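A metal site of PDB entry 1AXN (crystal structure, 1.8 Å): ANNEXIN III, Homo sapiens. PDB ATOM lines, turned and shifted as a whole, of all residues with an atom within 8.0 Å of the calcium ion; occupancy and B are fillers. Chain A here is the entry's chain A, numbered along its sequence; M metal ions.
Residues that only touch the calcium ion: Thr 36. Five residues have an atom within 4 Å of the calcium ion: Ile 31, Gly 33, Gly 35, Thr 36 and Asp 75. The nearest printed residue that does not touch the calcium ion is Ile 34 (4.2 Å).
OD2 of Asp 75 lies close to OG1 of Thr 36 (2.4 Å).
The calcium ion is bound by O of Gly 35, 2.2 Å away. The calcium ion is bound by O of Ile 31 (2.3 Å). The backbone carbonyl oxygen (O) of Gly 33 binds the calcium ion, at 2.6 Å. The calcium ion is bound by OD2 of Asp 75 (2.7 Å). Slightly farther from the calcium ion lies OD1 of Asp 75 (3.1 Å).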
ATOM      1  N   GLN A  28      -8.956  17.243  -1.790  1.00  0.00           N
ATOM      2  CA  GLN A  28     -10.265  17.423  -1.157  1.00  0.00           C
ATOM      3  C   GLN A  28     -10.420  16.547   0.072  1.00  0.00           C
ATOM      4  O   GLN A  28     -10.830  17.045   1.116  1.00  0.00           O
ATOM      5  CB  GLN A  28     -11.360  17.175  -2.172  1.00  0.00           C
ATOM      6  CG  GLN A  28     -12.689  16.720  -1.550  1.00  0.00           C
ATOM      7  CD  GLN A  28     -13.458  17.914  -1.061  1.00  0.00           C
ATOM      8  OE1 GLN A  28     -14.580  17.778  -0.580  1.00  0.00           O
ATOM      9  NE2 GLN A  28     -12.860  19.094  -1.184  1.00  0.00           N
ATOM     10  N   LYS A  29     -10.094  15.271  -0.012  1.00  0.00           N
ATOM     11  CA  LYS A  29     -10.232  14.391   1.135  1.00  0.00           C
ATOM     12  C   LYS A  29      -9.355  14.901   2.276  1.00  0.00           C
ATOM     13  O   LYS A  29      -9.712  14.854   3.461  1.00  0.00           O
ATOM     14  CB  LYS A  29      -9.950  12.950   0.737  1.00  0.00           C
ATOM     15  CG  LYS A  29      -8.743  12.218   1.213  1.00  0.00           C
ATOM     16  CD  LYS A  29      -7.531  12.274   0.298  1.00  0.00           C
ATOM     17  CE  LYS A  29      -6.242  12.349   1.100  1.00  0.00           C
ATOM     18  NZ  LYS A  29      -5.010  12.592   0.340  1.00  0.00           N
ATOM     19  N   ALA A  30      -8.171  15.406   1.954  1.00  0.00           N
ATOM     20  CA  ALA A  30      -7.198  15.919   2.893  1.00  0.00           C
ATOM     21  C   ALA A  30      -7.650  17.122   3.705  1.00  0.00           C
ATOM     22  O   ALA A  30      -7.183  17.244   4.848  1.00  0.00           O
ATOM     23  CB  ALA A  30      -5.888  16.204   2.158  1.00  0.00           C
ATOM     24  N   ILE A  31      -8.500  17.994   3.185  1.00  0.00           N
ATOM     25  CA  ILE A  31      -8.887  19.147   4.000  1.00  0.00           C
ATOM     26  C   ILE A  31     -10.304  19.010   4.512  1.00  0.00           C
ATOM     27  O   ILE A  31     -10.731  19.631   5.481  1.00  0.00           O
ATOM     28  CB  ILE A  31      -8.690  20.477   3.232  1.00  0.00           C
ATOM     29  CG1 ILE A  31      -9.724  20.630   2.127  1.00  0.00           C
ATOM     30  CG2 ILE A  31      -7.284  20.593   2.677  1.00  0.00           C
ATOM     31  CD1 ILE A  31      -9.502  21.792   1.206  1.00  0.00           C
ATOM     32  N   ARG A  32     -11.073  18.168   3.832  1.00  0.00           N
ATOM     33  CA  ARG A  32     -12.461  17.933   4.180  1.00  0.00           C
ATOM     34  C   ARG A  32     -12.647  17.509   5.629  1.00  0.00           C
ATOM     35  O   ARG A  32     -11.940  16.639   6.159  1.00  0.00           O
ATOM     36  CB  ARG A  32     -12.945  16.844   3.225  1.00  0.00           C
ATOM     37  CG  ARG A  32     -14.411  16.901   2.845  1.00  0.00           C
ATOM     38  CD  ARG A  32     -14.933  15.521   3.154  1.00  0.00           C
ATOM     39  NE  ARG A  32     -15.180  14.543   2.152  1.00  0.00           N
ATOM     40  CZ  ARG A  32     -15.581  14.563   0.906  1.00  0.00           C
ATOM     41  NH1 ARG A  32     -15.824  15.686   0.245  1.00  0.00           N
ATOM     42  NH2 ARG A  32     -15.726  13.405   0.274  1.00  0.00           N
ATOM     43  N   GLY A  33     -13.615  18.129   6.307  1.00  0.00           N
ATOM     44  CA  GLY A  33     -13.908  17.810   7.689  1.00  0.00           C
ATOM     45  C   GLY A  33     -13.041  18.400   8.769  1.00  0.00           C
ATOM     46  O   GLY A  33     -12.410  19.438   8.578  1.00  0.00           O
ATOM     47  N   ILE A  34     -13.001  17.739   9.934  1.00  0.00           N
ATOM     48  CA  ILE A  34     -12.195  18.268  11.028  1.00  0.00           C
ATOM     49  C   ILE A  34     -10.746  17.870  10.769  1.00  0.00           C
ATOM     50  O   ILE A  34     -10.451  16.752  10.383  1.00  0.00           O
ATOM     51  CB  ILE A  34     -12.584  17.835  12.456  1.00  0.00           C
ATOM     52  CG1 ILE A  34     -13.806  18.580  13.010  1.00  0.00           C
ATOM     53  CG2 ILE A  34     -11.438  18.040  13.466  1.00  0.00           C
ATOM     54  CD1 ILE A  34     -14.185  18.154  14.418  1.00  0.00           C
ATOM     55  N   GLY A  35      -9.877  18.835  11.011  1.00  0.00           N
ATOM     56  CA  GLY A  35      -8.459  18.577  10.831  1.00  0.00           C
ATOM     57  C   GLY A  35      -8.121  18.753   9.350  1.00  0.00           C
ATOM     58  O   GLY A  35      -8.935  19.101   8.501  1.00  0.00           O
ATOM     59  N   THR A  36      -6.844  18.471   9.148  1.00  0.00           N
ATOM     60  CA  THR A  36      -6.283  18.592   7.820  1.00  0.00           C
ATOM     61  C   THR A  36      -5.130  17.632   7.672  1.00  0.00           C
ATOM     62  O   THR A  36      -4.367  17.467   8.636  1.00  0.00           O
ATOM     63  CB  THR A  36      -5.746  20.042   7.692  1.00  0.00           C
ATOM     64  OG1 THR A  36      -6.843  20.905   8.019  1.00  0.00           O
ATOM     65  CG2 THR A  36      -5.205  20.295   6.301  1.00  0.00           C
ATOM     66  N   ASP A  37      -5.032  17.013   6.503  1.00  0.00           N
ATOM     67  CA  ASP A  37      -3.891  16.109   6.312  1.00  0.00           C
ATOM     68  C   ASP A  37      -2.842  17.019   5.639  1.00  0.00           C
ATOM     69  O   ASP A  37      -2.731  17.007   4.417  1.00  0.00           O
ATOM     70  CB  ASP A  37      -4.234  14.876   5.510  1.00  0.00           C
ATOM     71  CG  ASP A  37      -3.120  13.844   5.444  1.00  0.00           C
ATOM     72  OD1 ASP A  37      -1.996  14.087   5.924  1.00  0.00           O
ATOM     73  OD2 ASP A  37      -3.368  12.738   4.909  1.00  0.00           O
ATOM     74  N   ASP A  71     -10.053  27.117  -0.083  1.00  0.00           N
ATOM     75  CA  ASP A  71     -10.087  26.020   0.885  1.00  0.00           C
ATOM     76  C   ASP A  71      -8.782  25.984   1.662  1.00  0.00           C
ATOM     77  O   ASP A  71      -8.744  25.703   2.855  1.00  0.00           O
ATOM     78  CB  ASP A  71     -10.340  24.690   0.201  1.00  0.00           C
ATOM     79  CG  ASP A  71     -11.827  24.469   0.017  1.00  0.00           C
ATOM     80  OD1 ASP A  71     -12.614  25.335   0.433  1.00  0.00           O
ATOM     81  OD2 ASP A  71     -12.192  23.438  -0.558  1.00  0.00           O
ATOM     82  N   GLY A  74      -8.842  28.613   4.319  1.00  0.00           N
ATOM     83  CA  GLY A  74      -9.749  28.284   5.409  1.00  0.00           C
ATOM     84  C   GLY A  74      -9.225  27.233   6.371  1.00  0.00           C
ATOM     85  O   GLY A  74      -9.558  27.231   7.551  1.00  0.00           O
ATOM     86  N   ASP A  75      -8.383  26.325   5.878  1.00  0.00           N
ATOM     87  CA  ASP A  75      -7.822  25.257   6.676  1.00  0.00           C
ATOM     88  C   ASP A  75      -6.427  25.447   7.209  1.00  0.00           C
ATOM     89  O   ASP A  75      -6.142  24.937   8.282  1.00  0.00           O
ATOM     90  CB  ASP A  75      -7.679  23.997   5.778  1.00  0.00           C
ATOM     91  CG  ASP A  75      -8.701  22.917   6.076  1.00  0.00           C
ATOM     92  OD1 ASP A  75      -9.910  23.237   6.132  1.00  0.00           O
ATOM     93  OD2 ASP A  75      -8.291  21.744   6.247  1.00  0.00           O
ATOM     94  N   LEU A  76      -5.610  26.149   6.419  1.00  0.00           N
ATOM     95  CA  LEU A  76      -4.237  26.356   6.834  1.00  0.00           C
ATOM     96  C   LEU A  76      -4.019  27.714   7.522  1.00  0.00           C
ATOM     97  O   LEU A  76      -4.825  28.597   7.316  1.00  0.00           O
ATOM     98  CB  LEU A  76      -3.317  26.213   5.622  1.00  0.00           C
ATOM     99  CG  LEU A  76      -3.466  24.938   4.783  1.00  0.00           C
ATOM    100  CD1 LEU A  76      -2.309  24.825   3.796  1.00  0.00           C
ATOM    101  CD2 LEU A  76      -3.531  23.694   5.672  1.00  0.00           C
HETATM  102 CA    CA M   1     -10.322  20.509   7.548  1.00  0.00          CA
